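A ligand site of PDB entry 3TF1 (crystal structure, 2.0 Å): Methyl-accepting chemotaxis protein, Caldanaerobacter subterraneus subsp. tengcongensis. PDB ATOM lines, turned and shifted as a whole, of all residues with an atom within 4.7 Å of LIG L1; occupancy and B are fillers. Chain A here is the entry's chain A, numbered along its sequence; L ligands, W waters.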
ATOM      1  N   MET A   1      -4.080  15.801 -23.520  1.00  0.00           N
ATOM      2  CA  MET A   1      -5.259  14.949 -23.895  1.00  0.00           C
ATOM      3  C   MET A   1      -5.871  15.619 -25.117  1.00  0.00           C
ATOM      4  O   MET A   1      -5.943  16.839 -25.215  1.00  0.00           O
ATOM      5  CB  MET A   1      -6.283  14.874 -22.754  1.00  0.00           C
ATOM      6  CG  MET A   1      -7.269  13.674 -22.856  1.00  0.00           C
ATOM      7  SD  MET A   1      -6.319  12.119 -22.744  1.00  0.00           S
ATOM      8  CE  MET A   1      -5.836  12.284 -20.983  1.00  0.00           C
ATOM      9  N   LYS A   2      -6.317  14.826 -26.056  1.00  0.00           N
ATOM     10  CA  LYS A   2      -7.006  15.346 -27.204  1.00  0.00           C
ATOM     11  C   LYS A   2      -8.263  16.106 -26.773  1.00  0.00           C
ATOM     12  O   LYS A   2      -9.114  15.580 -26.027  1.00  0.00           O
ATOM     13  CB  LYS A   2      -7.419  14.201 -28.171  1.00  0.00           C
ATOM     14  CG  LYS A   2      -7.785  14.740 -29.580  1.00  0.00           C
ATOM     15  CD  LYS A   2      -7.951  13.627 -30.604  1.00  0.00           C
ATOM     16  CE  LYS A   2      -8.317  14.307 -31.974  1.00  0.00           C
ATOM     17  NZ  LYS A   2      -8.907  13.272 -32.964  1.00  0.00           N
ATOM     18  N   ILE A   5     -11.902  14.549 -26.684  1.00  0.00           N
ATOM     19  CA  ILE A   5     -12.248  13.642 -25.620  1.00  0.00           C
ATOM     20  C   ILE A   5     -12.468  14.393 -24.304  1.00  0.00           C
ATOM     21  O   ILE A   5     -13.396  14.102 -23.558  1.00  0.00           O
ATOM     22  CB  ILE A   5     -11.144  12.558 -25.466  1.00  0.00           C
ATOM     23  CG1 ILE A   5     -10.924  11.865 -26.831  1.00  0.00           C
ATOM     24  CG2 ILE A   5     -11.568  11.577 -24.424  1.00  0.00           C
ATOM     25  CD1 ILE A   5     -12.270  11.308 -27.511  1.00  0.00           C
ATOM     26  N   TRP A   9     -15.585  14.444 -21.542  1.00  0.00           N
ATOM     27  CA  TRP A   9     -15.528  14.325 -20.105  1.00  0.00           C
ATOM     28  C   TRP A   9     -16.339  15.437 -19.399  1.00  0.00           C
ATOM     29  O   TRP A   9     -16.905  15.201 -18.343  1.00  0.00           O
ATOM     30  CB  TRP A   9     -14.055  14.385 -19.605  1.00  0.00           C
ATOM     31  CG  TRP A   9     -13.277  13.155 -20.080  1.00  0.00           C
ATOM     32  CD1 TRP A   9     -13.830  12.025 -20.553  1.00  0.00           C
ATOM     33  CD2 TRP A   9     -11.864  13.002 -20.181  1.00  0.00           C
ATOM     34  NE1 TRP A   9     -12.859  11.118 -20.899  1.00  0.00           N
ATOM     35  CE2 TRP A   9     -11.631  11.688 -20.681  1.00  0.00           C
ATOM     36  CE3 TRP A   9     -10.773  13.815 -19.866  1.00  0.00           C
ATOM     37  CZ2 TRP A   9     -10.345  11.185 -20.927  1.00  0.00           C
ATOM     38  CZ3 TRP A   9      -9.460  13.303 -20.076  1.00  0.00           C
ATOM     39  CH2 TRP A   9      -9.264  11.987 -20.638  1.00  0.00           C
ATOM     40  N   ILE A  75     -18.903   6.056 -22.094  1.00  0.00           N
ATOM     41  CA  ILE A  75     -19.317   5.194 -23.201  1.00  0.00           C
ATOM     42  C   ILE A  75     -20.627   5.754 -23.802  1.00  0.00           C
ATOM     43  O   ILE A  75     -20.721   5.930 -25.019  1.00  0.00           O
ATOM     44  CB  ILE A  75     -19.511   3.722 -22.758  1.00  0.00           C
ATOM     45  CG1 ILE A  75     -18.123   3.084 -22.419  1.00  0.00           C
ATOM     46  CG2 ILE A  75     -20.210   2.904 -23.853  1.00  0.00           C
ATOM     47  CD1 ILE A  75     -17.059   3.223 -23.569  1.00  0.00           C
ATOM     48  N   PHE A  78     -19.909   8.842 -25.711  1.00  0.00           N
ATOM     49  CA  PHE A  78     -19.269   8.516 -26.982  1.00  0.00           C
ATOM     50  C   PHE A  78     -20.353   8.009 -27.976  1.00  0.00           C
ATOM     51  O   PHE A  78     -20.332   8.340 -29.181  1.00  0.00           O
ATOM     52  CB  PHE A  78     -18.207   7.406 -26.845  1.00  0.00           C
ATOM     53  CG  PHE A  78     -16.846   7.843 -26.299  1.00  0.00           C
ATOM     54  CD1 PHE A  78     -16.328   9.092 -26.534  1.00  0.00           C
ATOM     55  CD2 PHE A  78     -16.059   6.909 -25.581  1.00  0.00           C
ATOM     56  CE1 PHE A  78     -15.061   9.458 -26.017  1.00  0.00           C
ATOM     57  CE2 PHE A  78     -14.789   7.257 -25.061  1.00  0.00           C
ATOM     58  CZ  PHE A  78     -14.277   8.532 -25.317  1.00  0.00           C
ATOM     59  N   PHE A  82     -20.275  10.181 -31.180  1.00  0.00           N
ATOM     60  CA  PHE A  82     -19.434   9.515 -32.221  1.00  0.00           C
ATOM     61  C   PHE A  82     -20.077   8.157 -32.521  1.00  0.00           C
ATOM     62  O   PHE A  82     -19.455   7.128 -32.356  1.00  0.00           O
ATOM     63  CB  PHE A  82     -17.950   9.340 -31.788  1.00  0.00           C
ATOM     64  CG  PHE A  82     -17.345  10.537 -31.118  1.00  0.00           C
ATOM     65  CD1 PHE A  82     -17.469  11.809 -31.682  1.00  0.00           C
ATOM     66  CD2 PHE A  82     -16.679  10.400 -29.894  1.00  0.00           C
ATOM     67  CE1 PHE A  82     -16.959  12.927 -31.057  1.00  0.00           C
ATOM     68  CE2 PHE A  82     -16.148  11.494 -29.251  1.00  0.00           C
ATOM     69  CZ  PHE A  82     -16.278  12.787 -29.825  1.00  0.00           C
ATOM     70  N   TYR A  85     -18.694   4.713 -34.287  1.00  0.00           N
ATOM     71  CA  TYR A  85     -17.861   3.666 -33.682  1.00  0.00           C
ATOM     72  C   TYR A  85     -18.688   2.510 -33.107  1.00  0.00           C
ATOM     73  O   TYR A  85     -18.130   1.445 -32.868  1.00  0.00           O
ATOM     74  CB  TYR A  85     -16.930   4.246 -32.621  1.00  0.00           C
ATOM     75  CG  TYR A  85     -15.941   5.166 -33.259  1.00  0.00           C
ATOM     76  CD1 TYR A  85     -14.779   4.659 -33.860  1.00  0.00           C
ATOM     77  CD2 TYR A  85     -16.192   6.541 -33.342  1.00  0.00           C
ATOM     78  CE1 TYR A  85     -13.884   5.483 -34.495  1.00  0.00           C
ATOM     79  CE2 TYR A  85     -15.295   7.381 -33.947  1.00  0.00           C
ATOM     80  CZ  TYR A  85     -14.118   6.838 -34.524  1.00  0.00           C
ATOM     81  OH  TYR A  85     -13.212   7.647 -35.146  1.00  0.00           O
ATOM     82  N   PHE A  86     -19.997   2.699 -32.939  1.00  0.00           N
ATOM     83  CA  PHE A  86     -20.867   1.703 -32.307  1.00  0.00           C
ATOM     84  C   PHE A  86     -21.772   0.973 -33.326  1.00  0.00           C
ATOM     85  O   PHE A  86     -22.048  -0.184 -33.183  1.00  0.00           O
ATOM     86  CB  PHE A  86     -21.731   2.372 -31.214  1.00  0.00           C
ATOM     87  CG  PHE A  86     -20.887   2.943 -30.058  1.00  0.00           C
ATOM     88  CD1 PHE A  86     -20.655   2.197 -28.913  1.00  0.00           C
ATOM     89  CD2 PHE A  86     -20.275   4.192 -30.175  1.00  0.00           C
ATOM     90  CE1 PHE A  86     -19.837   2.712 -27.850  1.00  0.00           C
ATOM     91  CE2 PHE A  86     -19.481   4.727 -29.109  1.00  0.00           C
ATOM     92  CZ  PHE A  86     -19.260   3.962 -27.960  1.00  0.00           C
ATOM     93  N   PHE A  94     -15.946  -4.257 -30.967  1.00  0.00           N
ATOM     94  CA  PHE A  94     -15.714  -2.928 -30.474  1.00  0.00           C
ATOM     95  C   PHE A  94     -14.401  -2.925 -29.662  1.00  0.00           C
ATOM     96  O   PHE A  94     -13.514  -2.150 -29.966  1.00  0.00           O
ATOM     97  CB  PHE A  94     -16.875  -2.515 -29.636  1.00  0.00           C
ATOM     98  CG  PHE A  94     -16.768  -1.123 -29.039  1.00  0.00           C
ATOM     99  CD1 PHE A  94     -17.131  -0.006 -29.783  1.00  0.00           C
ATOM    100  CD2 PHE A  94     -16.285  -0.947 -27.764  1.00  0.00           C
ATOM    101  CE1 PHE A  94     -17.074   1.304 -29.218  1.00  0.00           C
ATOM    102  CE2 PHE A  94     -16.234   0.322 -27.185  1.00  0.00           C
ATOM    103  CZ  PHE A  94     -16.605   1.444 -27.925  1.00  0.00           C
ATOM    104  N   LEU A  95     -14.275  -3.826 -28.678  1.00  0.00           N
ATOM    105  CA  LEU A  95     -13.073  -3.893 -27.857  1.00  0.00           C
ATOM    106  C   LEU A  95     -11.792  -4.160 -28.667  1.00  0.00           C
ATOM    107  O   LEU A  95     -10.755  -3.515 -28.450  1.00  0.00           O
ATOM    108  CB  LEU A  95     -13.229  -4.942 -26.756  1.00  0.00           C
ATOM    109  CG  LEU A  95     -14.264  -4.551 -25.692  1.00  0.00           C
ATOM    110  CD1 LEU A  95     -14.468  -5.723 -24.713  1.00  0.00           C
ATOM    111  CD2 LEU A  95     -13.925  -3.238 -24.943  1.00  0.00           C
ATOM    112  N   MET A  98     -10.203  -1.080 -30.527  1.00  0.00           N
ATOM    113  CA  MET A  98      -9.885   0.136 -29.767  1.00  0.00           C
ATOM    114  C   MET A  98      -8.437   0.566 -29.962  1.00  0.00           C
ATOM    115  O   MET A  98      -8.159   1.785 -30.131  1.00  0.00           O
ATOM    116  CB  MET A  98     -10.144  -0.100 -28.292  1.00  0.00           C
ATOM    117  CG  MET A  98     -11.648   0.011 -27.988  1.00  0.00           C
ATOM    118  SD  MET A  98     -12.415   1.612 -28.479  1.00  0.00           S
ATOM    119  CE  MET A  98     -13.062   1.302 -30.111  1.00  0.00           C
ATOM    120  N   VAL A 101      -8.237   2.330 -33.346  1.00  0.00           N
ATOM    121  CA  VAL A 101      -8.980   3.559 -33.211  1.00  0.00           C
ATOM    122  C   VAL A 101      -8.148   4.643 -32.474  1.00  0.00           C
ATOM    123  O   VAL A 101      -8.063   5.801 -32.932  1.00  0.00           O
ATOM    124  CB  VAL A 101     -10.331   3.313 -32.458  1.00  0.00           C
ATOM    125  CG1 VAL A 101     -10.985   4.646 -32.082  1.00  0.00           C
ATOM    126  CG2 VAL A 101     -11.271   2.481 -33.363  1.00  0.00           C
ATOM    127  N   HIS A 102      -7.488   4.268 -31.394  1.00  0.00           N
ATOM    128  CA  HIS A 102      -6.772   5.245 -30.609  1.00  0.00           C
ATOM    129  C   HIS A 102      -5.536   5.802 -31.360  1.00  0.00           C
ATOM    130  O   HIS A 102      -5.217   6.986 -31.200  1.00  0.00           O
ATOM    131  CB  HIS A 102      -6.443   4.711 -29.201  1.00  0.00           C
ATOM    132  CG  HIS A 102      -7.621   4.775 -28.267  1.00  0.00           C
ATOM    133  ND1 HIS A 102      -8.707   3.938 -28.401  1.00  0.00           N
ATOM    134  CD2 HIS A 102      -7.921   5.626 -27.239  1.00  0.00           C
ATOM    135  CE1 HIS A 102      -9.596   4.208 -27.452  1.00  0.00           C
ATOM    136  NE2 HIS A 102      -9.133   5.229 -26.741  1.00  0.00           N
ATOM    137  N   LEU A 105      -6.929   8.155 -34.265  1.00  0.00           N
ATOM    138  CA  LEU A 105      -7.560   9.421 -33.836  1.00  0.00           C
ATOM    139  C   LEU A 105      -6.534  10.369 -33.254  1.00  0.00           C
ATOM    140  O   LEU A 105      -6.861  11.514 -32.949  1.00  0.00           O
ATOM    141  CB  LEU A 105      -8.667   9.158 -32.821  1.00  0.00           C
ATOM    142  CG  LEU A 105     -10.002   8.642 -33.368  1.00  0.00           C
ATOM    143  CD1 LEU A 105     -10.952   8.456 -32.219  1.00  0.00           C
ATOM    144  CD2 LEU A 105     -10.642   9.592 -34.440  1.00  0.00           C
ATOM    145  N   THR A 106      -5.307   9.902 -33.081  1.00  0.00           N
ATOM    146  CA  THR A 106      -4.220  10.780 -32.662  1.00  0.00           C
ATOM    147  C   THR A 106      -3.069  10.925 -33.689  1.00  0.00           C
ATOM    148  O   THR A 106      -2.100  11.630 -33.429  1.00  0.00           O
ATOM    149  CB  THR A 106      -3.618  10.321 -31.340  1.00  0.00           C
ATOM    150  OG1 THR A 106      -3.130   8.978 -31.448  1.00  0.00           O
ATOM    151  CG2 THR A 106      -4.660  10.406 -30.215  1.00  0.00           C
ATOM    152  N   THR A 113       0.702  10.615 -27.804  1.00  0.00           N
ATOM    153  CA  THR A 113       0.953   9.518 -26.901  1.00  0.00           C
ATOM    154  C   THR A 113      -0.364   8.842 -26.528  1.00  0.00           C
ATOM    155  O   THR A 113      -0.789   8.863 -25.378  1.00  0.00           O
ATOM    156  CB  THR A 113       1.654   9.994 -25.618  1.00  0.00           C
ATOM    157  OG1 THR A 113       0.906  11.099 -25.100  1.00  0.00           O
ATOM    158  CG2 THR A 113       3.098  10.479 -25.887  1.00  0.00           C
ATOM    159  N   PRO A 114      -1.039   8.234 -27.530  1.00  0.00           N
ATOM    160  CA  PRO A 114      -2.270   7.533 -27.187  1.00  0.00           C
ATOM    161  C   PRO A 114      -2.001   6.349 -26.241  1.00  0.00           C
ATOM    162  O   PRO A 114      -0.884   5.771 -26.264  1.00  0.00           O
ATOM    163  CB  PRO A 114      -2.762   6.992 -28.546  1.00  0.00           C
ATOM    164  CG  PRO A 114      -1.449   6.873 -29.389  1.00  0.00           C
ATOM    165  CD  PRO A 114      -0.694   8.117 -28.965  1.00  0.00           C
ATOM    166  N   PRO A 115      -3.008   5.966 -25.424  1.00  0.00           N
ATOM    167  CA  PRO A 115      -2.872   4.699 -24.655  1.00  0.00           C
ATOM    168  C   PRO A 115      -2.845   3.552 -25.678  1.00  0.00           C
ATOM    169  O   PRO A 115      -3.473   3.689 -26.716  1.00  0.00           O
ATOM    170  CB  PRO A 115      -4.143   4.650 -23.839  1.00  0.00           C
ATOM    171  CG  PRO A 115      -5.159   5.482 -24.713  1.00  0.00           C
ATOM    172  CD  PRO A 115      -4.369   6.534 -25.415  1.00  0.00           C
ATOM    173  N   LEU A 117      -3.995  -0.322 -26.286  1.00  0.00           N
ATOM    174  CA  LEU A 117      -5.067  -1.130 -25.721  1.00  0.00           C
ATOM    175  C   LEU A 117      -5.130  -2.482 -26.432  1.00  0.00           C
ATOM    176  O   LEU A 117      -6.221  -2.944 -26.760  1.00  0.00           O
ATOM    177  CB  LEU A 117      -6.377  -0.377 -25.947  1.00  0.00           C
ATOM    178  CG  LEU A 117      -6.414   1.022 -25.398  1.00  0.00           C
ATOM    179  CD1 LEU A 117      -7.539   1.810 -26.101  1.00  0.00           C
ATOM    180  CD2 LEU A 117      -6.578   0.960 -23.875  1.00  0.00           C
ATOM    181  N   MET A 129      -6.717  -8.040 -22.606  1.00  0.00           N
ATOM    182  CA  MET A 129      -6.533  -6.706 -23.108  1.00  0.00           C
ATOM    183  C   MET A 129      -5.562  -6.019 -22.181  1.00  0.00           C
ATOM    184  O   MET A 129      -5.712  -6.099 -20.968  1.00  0.00           O
ATOM    185  CB  MET A 129      -7.889  -5.973 -23.152  1.00  0.00           C
ATOM    186  CG  MET A 129      -7.852  -4.591 -23.736  1.00  0.00           C
ATOM    187  SD  MET A 129      -9.512  -3.919 -24.025  1.00  0.00           S
ATOM    188  CE  MET A 129      -9.211  -2.644 -25.198  1.00  0.00           C
ATOM    189  N   TYR A 131      -3.888  -2.456 -21.142  1.00  0.00           N
ATOM    190  CA  TYR A 131      -3.746  -1.019 -21.182  1.00  0.00           C
ATOM    191  C   TYR A 131      -2.284  -0.643 -20.928  1.00  0.00           C
ATOM    192  O   TYR A 131      -1.666  -1.071 -19.947  1.00  0.00           O
ATOM    193  CB  TYR A 131      -4.598  -0.443 -20.047  1.00  0.00           C
ATOM    194  CG  TYR A 131      -4.328   0.998 -19.698  1.00  0.00           C
ATOM    195  CD1 TYR A 131      -4.817   2.027 -20.508  1.00  0.00           C
ATOM    196  CD2 TYR A 131      -3.597   1.331 -18.564  1.00  0.00           C
ATOM    197  CE1 TYR A 131      -4.578   3.366 -20.183  1.00  0.00           C
ATOM    198  CE2 TYR A 131      -3.386   2.686 -18.213  1.00  0.00           C
ATOM    199  CZ  TYR A 131      -3.871   3.686 -19.027  1.00  0.00           C
ATOM    200  OH  TYR A 131      -3.644   5.005 -18.698  1.00  0.00           O
ATOM    201  N   SER A 133       0.138   2.913 -20.913  1.00  0.00           N
ATOM    202  CA  SER A 133       0.129   4.359 -21.112  1.00  0.00           C
ATOM    203  C   SER A 133       0.940   5.007 -20.013  1.00  0.00           C
ATOM    204  O   SER A 133       0.904   4.551 -18.892  1.00  0.00           O
ATOM    205  CB  SER A 133      -1.316   4.931 -21.016  1.00  0.00           C
ATOM    206  OG  SER A 133      -1.230   6.362 -20.932  1.00  0.00           O
ATOM    207  N   ARG A 135       0.030   7.618 -18.682  1.00  0.00           N
ATOM    208  CA  ARG A 135      -0.918   8.433 -17.919  1.00  0.00           C
ATOM    209  C   ARG A 135      -1.503   7.792 -16.680  1.00  0.00           C
ATOM    210  O   ARG A 135      -2.138   8.467 -15.881  1.00  0.00           O
ATOM    211  CB  ARG A 135      -2.083   8.912 -18.831  1.00  0.00           C
ATOM    212  CG  ARG A 135      -1.597   9.847 -19.898  1.00  0.00           C
ATOM    213  CD  ARG A 135      -2.781  10.451 -20.594  1.00  0.00           C
ATOM    214  NE  ARG A 135      -2.381  11.337 -21.657  1.00  0.00           N
ATOM    215  CZ  ARG A 135      -2.492  11.013 -22.947  1.00  0.00           C
ATOM    216  NH1 ARG A 135      -2.946   9.816 -23.327  1.00  0.00           N
ATOM    217  NH2 ARG A 135      -2.093  11.889 -23.855  1.00  0.00           N
ATOM    218  N   MET A 137      -4.164   5.774 -16.101  1.00  0.00           N
ATOM    219  CA  MET A 137      -5.590   6.047 -15.911  1.00  0.00           C
ATOM    220  C   MET A 137      -6.347   4.725 -15.768  1.00  0.00           C
ATOM    221  O   MET A 137      -7.257   4.415 -16.534  1.00  0.00           O
ATOM    222  CB  MET A 137      -6.073   6.956 -17.036  1.00  0.00           C
ATOM    223  CG  MET A 137      -5.373   8.367 -16.961  1.00  0.00           C
ATOM    224  SD  MET A 137      -5.885   9.363 -18.390  1.00  0.00           S
ATOM    225  CE  MET A 137      -7.594   9.644 -17.922  1.00  0.00           C
ATOM    226  N   TYR A 140     -10.295   4.804 -15.192  1.00  0.00           N
ATOM    227  CA  TYR A 140     -10.984   5.230 -16.388  1.00  0.00           C
ATOM    228  C   TYR A 140     -11.056   4.028 -17.397  1.00  0.00           C
ATOM    229  O   TYR A 140     -12.135   3.690 -17.880  1.00  0.00           O
ATOM    230  CB  TYR A 140     -10.290   6.473 -16.995  1.00  0.00           C
ATOM    231  CG  TYR A 140     -10.947   6.993 -18.228  1.00  0.00           C
ATOM    232  CD1 TYR A 140     -12.274   7.386 -18.203  1.00  0.00           C
ATOM    233  CD2 TYR A 140     -10.231   7.093 -19.443  1.00  0.00           C
ATOM    234  CE1 TYR A 140     -12.913   7.849 -19.356  1.00  0.00           C
ATOM    235  CE2 TYR A 140     -10.851   7.569 -20.604  1.00  0.00           C
ATOM    236  CZ  TYR A 140     -12.197   7.915 -20.553  1.00  0.00           C
ATOM    237  OH  TYR A 140     -12.831   8.384 -21.658  1.00  0.00           O
ATOM    238  N   PHE A 141      -9.939   3.365 -17.623  1.00  0.00           N
ATOM    239  CA  PHE A 141      -9.877   2.194 -18.506  1.00  0.00           C
ATOM    240  C   PHE A 141     -10.893   1.106 -18.040  1.00  0.00           C
ATOM    241  O   PHE A 141     -11.656   0.584 -18.855  1.00  0.00           O
ATOM    242  CB  PHE A 141      -8.410   1.655 -18.509  1.00  0.00           C
ATOM    243  CG  PHE A 141      -8.247   0.275 -19.121  1.00  0.00           C
ATOM    244  CD1 PHE A 141      -8.327   0.104 -20.498  1.00  0.00           C
ATOM    245  CD2 PHE A 141      -7.999  -0.841 -18.319  1.00  0.00           C
ATOM    246  CE1 PHE A 141      -8.096  -1.188 -21.099  1.00  0.00           C
ATOM    247  CE2 PHE A 141      -7.829  -2.133 -18.885  1.00  0.00           C
ATOM    248  CZ  PHE A 141      -7.896  -2.310 -20.279  1.00  0.00           C
ATOM    249  N   LEU A 144     -14.463   2.274 -18.579  1.00  0.00           N
ATOM    250  CA  LEU A 144     -14.909   2.230 -19.976  1.00  0.00           C
ATOM    251  C   LEU A 144     -15.333   0.778 -20.414  1.00  0.00           C
ATOM    252  O   LEU A 144     -16.331   0.572 -21.131  1.00  0.00           O
ATOM    253  CB  LEU A 144     -13.817   2.771 -20.912  1.00  0.00           C
ATOM    254  CG  LEU A 144     -13.585   4.284 -20.838  1.00  0.00           C
ATOM    255  CD1 LEU A 144     -12.126   4.560 -21.391  1.00  0.00           C
ATOM    256  CD2 LEU A 144     -14.703   5.072 -21.600  1.00  0.00           C
ATOM    257  N   ILE A 145     -14.577  -0.210 -19.946  1.00  0.00           N
ATOM    258  CA  ILE A 145     -14.924  -1.594 -20.215  1.00  0.00           C
ATOM    259  C   ILE A 145     -16.280  -1.895 -19.617  1.00  0.00           C
ATOM    260  O   ILE A 145     -17.137  -2.517 -20.258  1.00  0.00           O
ATOM    261  CB  ILE A 145     -13.858  -2.524 -19.677  1.00  0.00           C
ATOM    262  CG1 ILE A 145     -12.564  -2.236 -20.442  1.00  0.00           C
ATOM    263  CG2 ILE A 145     -14.316  -4.129 -19.821  1.00  0.00           C
ATOM    264  CD1 ILE A 145     -11.332  -2.949 -19.881  1.00  0.00           C
ATOM    265  N   SER A 148     -18.868  -0.245 -21.614  1.00  0.00           N
ATOM    266  CA  SER A 148     -19.059  -0.912 -22.905  1.00  0.00           C
ATOM    267  C   SER A 148     -19.996  -2.132 -22.753  1.00  0.00           C
ATOM    268  O   SER A 148     -20.902  -2.351 -23.553  1.00  0.00           O
ATOM    269  CB  SER A 148     -17.702  -1.297 -23.528  1.00  0.00           C
ATOM    270  OG  SER A 148     -17.007  -0.103 -23.907  1.00  0.00           O
HETATM  271  C1  LIG L   1      -8.277   8.392 -24.268  1.00  0.00           C
HETATM  272  C2  LIG L   1     -10.967   7.983 -28.308  1.00  0.00           C
HETATM  273  C3  LIG L   1     -13.263   4.225 -26.209  1.00  0.00           C
HETATM  274  C4  LIG L   1      -9.396   3.723 -23.338  1.00  0.00           C
HETATM  275  C5  LIG L   1      -8.738   8.593 -25.570  1.00  0.00           C
HETATM  276  C6  LIG L   1      -8.275   9.572 -26.541  1.00  0.00           C
HETATM  277  C7  LIG L   1      -9.014   9.417 -27.650  1.00  0.00           C
HETATM  278  C8  LIG L   1      -9.977   8.403 -27.420  1.00  0.00           C
HETATM  279  C9  LIG L   1      -8.829  10.229 -28.949  1.00  0.00           C
HETATM  280  C10 LIG L   1      -7.130  10.610 -26.383  1.00  0.00           C
HETATM  281  C11 LIG L   1      -5.736   9.976 -26.444  1.00  0.00           C
HETATM  282  C12 LIG L   1      -4.617  11.036 -26.361  1.00  0.00           C
HETATM  283  O1  LIG L   1      -3.430  10.618 -26.269  1.00  0.00           O
HETATM  284  O2  LIG L   1      -4.877  12.283 -26.372  1.00  0.00           O
HETATM  285  C13 LIG L   1     -11.912   7.023 -27.996  1.00  0.00           C
HETATM  286  C14 LIG L   1     -13.106   6.720 -28.770  1.00  0.00           C
HETATM  287  C15 LIG L   1     -13.731   5.693 -28.169  1.00  0.00           C
HETATM  288  C16 LIG L   1     -12.935   5.264 -27.041  1.00  0.00           C
HETATM  289  C17 LIG L   1     -13.532   7.543 -29.997  1.00  0.00           C
HETATM  290  C18 LIG L   1     -15.039   4.952 -28.529  1.00  0.00           C
HETATM  291  C19 LIG L   1     -15.811   5.384 -29.522  1.00  0.00           C
HETATM  292  C20 LIG L   1     -12.339   3.673 -25.344  1.00  0.00           C
HETATM  293  C21 LIG L   1     -12.351   2.344 -24.737  1.00  0.00           C
HETATM  294  C22 LIG L   1     -11.274   2.252 -23.961  1.00  0.00           C
HETATM  295  C23 LIG L   1     -10.530   3.447 -24.064  1.00  0.00           C
HETATM  296  C24 LIG L   1     -13.441   1.268 -24.891  1.00  0.00           C
HETATM  297  C25 LIG L   1     -10.848   1.054 -23.100  1.00  0.00           C
HETATM  298  C26 LIG L   1     -11.213  -0.140 -23.519  1.00  0.00           C
HETATM  299  C27 LIG L   1      -8.930   5.003 -23.158  1.00  0.00           C
HETATM  300  C28 LIG L   1      -8.136   5.467 -22.002  1.00  0.00           C
HETATM  301  C29 LIG L   1      -7.790   6.925 -22.278  1.00  0.00           C
HETATM  302  C30 LIG L   1      -8.363   7.189 -23.592  1.00  0.00           C
HETATM  303  C31 LIG L   1      -7.792   4.627 -20.756  1.00  0.00           C
HETATM  304  C32 LIG L   1      -7.010   7.960 -21.384  1.00  0.00           C
HETATM  305  C33 LIG L   1      -5.644   8.297 -22.035  1.00  0.00           C
HETATM  306  C34 LIG L   1      -4.597   7.410 -21.368  1.00  0.00           C
HETATM  307  O3  LIG L   1      -4.947   6.499 -20.567  1.00  0.00           O
HETATM  308  O4  LIG L   1      -3.383   7.585 -21.705  1.00  0.00           O
HETATM  309  N1  LIG L   1      -9.742   7.870 -26.177  1.00  0.00           N
HETATM  310  N2  LIG L   1     -11.858   6.132 -26.935  1.00  0.00           N
HETATM  311  N3  LIG L   1     -11.186   4.317 -24.899  1.00  0.00           N
HETATM  312  N4  LIG L   1      -8.996   6.039 -24.084  1.00  0.00           N
HETATM  313 FE1  LIG L   1     -10.486   6.100 -25.478  1.00  0.00          FE
HETATM  314  O1  LG2 L   2     -11.761   6.972 -24.220  1.00  0.00           O
HETATM  315  O2  LG2 L   2     -11.094   8.379 -23.797  1.00  0.00           O
HETATM  316  O   HOH W   1      -2.891  14.027 -26.064  1.00  0.00           O
HETATM  317  O   HOH W   2      -1.744  12.175 -27.611  1.00  0.00           O
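OH of Tyr 131 sits at hydrogen-bond distance from O3 of LIG L1, 2.7 Å away.
The side-chain hydroxyl (OH) of Tyr 140 lies within hydrogen-bond range of an oxygen (O2) of LG2 L2 (2.8 Å).
The guanidinium group (NH1) of Arg 135 lies within salt-bridge range of an oxygen (O4) of LIG L1, 2.8 Å away.
An oxygen (O2) of LIG L1 is in hydrogen-bond range of the backbone NH (N) of Lys 2.
A ring nitrogen (NE2) of His 102 binds an iron atom (FE1) of LIG L1, 2.0 Å away.
O4 of LIG L1 lies within hydrogen-bond range of OG of Ser 133 (2.6 Å).
An iron atom (FE1) of LIG L1 is bound by an oxygen (O1) of LG2 L2.
The backbone NH (N) of Arg 135 is in hydrogen-bond range of the side-chain hydroxyl (OG) of Ser 133, at 2.9 Å.
The backbone NH (N) of Met 137 lies within hydrogen-bond range of the side-chain hydroxyl (OH) of Tyr 131 (2.8 Å).
A ring nitrogen (ND1) of His 102 lies within hydrogen-bond range of the backbone carbonyl oxygen of Met 98 (2.8 Å).
OG1 of Thr 106 sits at hydrogen-bond distance from O of His 102 (2.9 Å).
NH1 of Arg 135 lies within hydrogen-bond range of O of Thr 113.
NZ of Lys 2 sits at hydrogen-bond distance from O of Leu 105.
The side-chain hydroxyl of Tyr 140 is in hydrogen-bond range of the indole nitrogen of Trp 9 (2.8 Å).
The backbone carbonyl oxygen of Leu 144 sits at hydrogen-bond distance from the side-chain hydroxyl of Ser 148 (2.9 Å).
O of Thr 113 lies close to O1 of LIG L1, 3.3 Å away.
An oxygen (O3) of LIG L1 lies close to the side-chain sulfur of Met 137, at 3.7 Å.
Met 1 touches LIG L1.
Ile 5 touches LIG L1.
CE2 of Phe 78 touches C16 of LIG L1, at 3.4 Å.
Tyr 85 touches LIG L1 (CB to C19, 3.5 Å).
CE2 of Phe 86 touches C19 of LIG L1, at 3.8 Å.
Phe 94 touches LIG L1 (CE2 to C24, 3.7 Å).
Met 98 touches LIG L1 (SD to C3, 3.6 Å).
Leu 105 touches LIG L1 (CD1 to C17, 3.5 Å).
Thr 106 touches LIG L1.
Pro 114 touches LIG L1.
CB of Pro 115 touches O4 of LIG L1 (3.7 Å).
Leu 117 touches LIG L1 (CD1 to C4, 3.8 Å).
Met 129 touches LIG L1 (CE to C26, 3.6 Å).
CE2 of Tyr 140 touches C29 of LIG L1, 3.5 Å away.
Phe 141 touches LIG L1 (CD1 to C25, 3.7 Å).
Leu 144 touches LIG L1 (CD1 to C23, 3.3 Å).
CG1 of Ile 145 touches C26 of LIG L1 (3.96 Å).
Ser 148 touches LIG L1.
Hydrophobic or aromatic side chains within 4 Å of LIG L1: Met 1, Ile 5, Phe 78, Tyr 85, Phe 86, Phe 94, Met 98, His 102, Leu 105, Pro 115, Leu 117, Met 129, Tyr 131, Met 137, Tyr 140, Phe 141, Leu 144 and Ile 145.
25 residues have an atom within 4 Å of LIG L1: Met 1, Lys 2, Ile 5, Phe 78, Tyr 85, Phe 86, Phe 94, Met 98, His 102, Leu 105, Thr 106, Thr 113, Pro 114, Pro 115, Leu 117, Met 129, Tyr 131, Ser 133, Arg 135, Met 137, Tyr 140, Phe 141, Leu 144, Ile 145 and Ser 148.
Water W2 bridges an oxygen (O1) of LIG L1 (2.7 Å) and the backbone NH of Thr 113 (2.9 Å).
Water W1 lies within hydrogen-bond range of O2 of LIG L1 (2.7 Å), NH2 of Arg 135 (3.2 Å) and N of Met 1 (3.3 Å).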
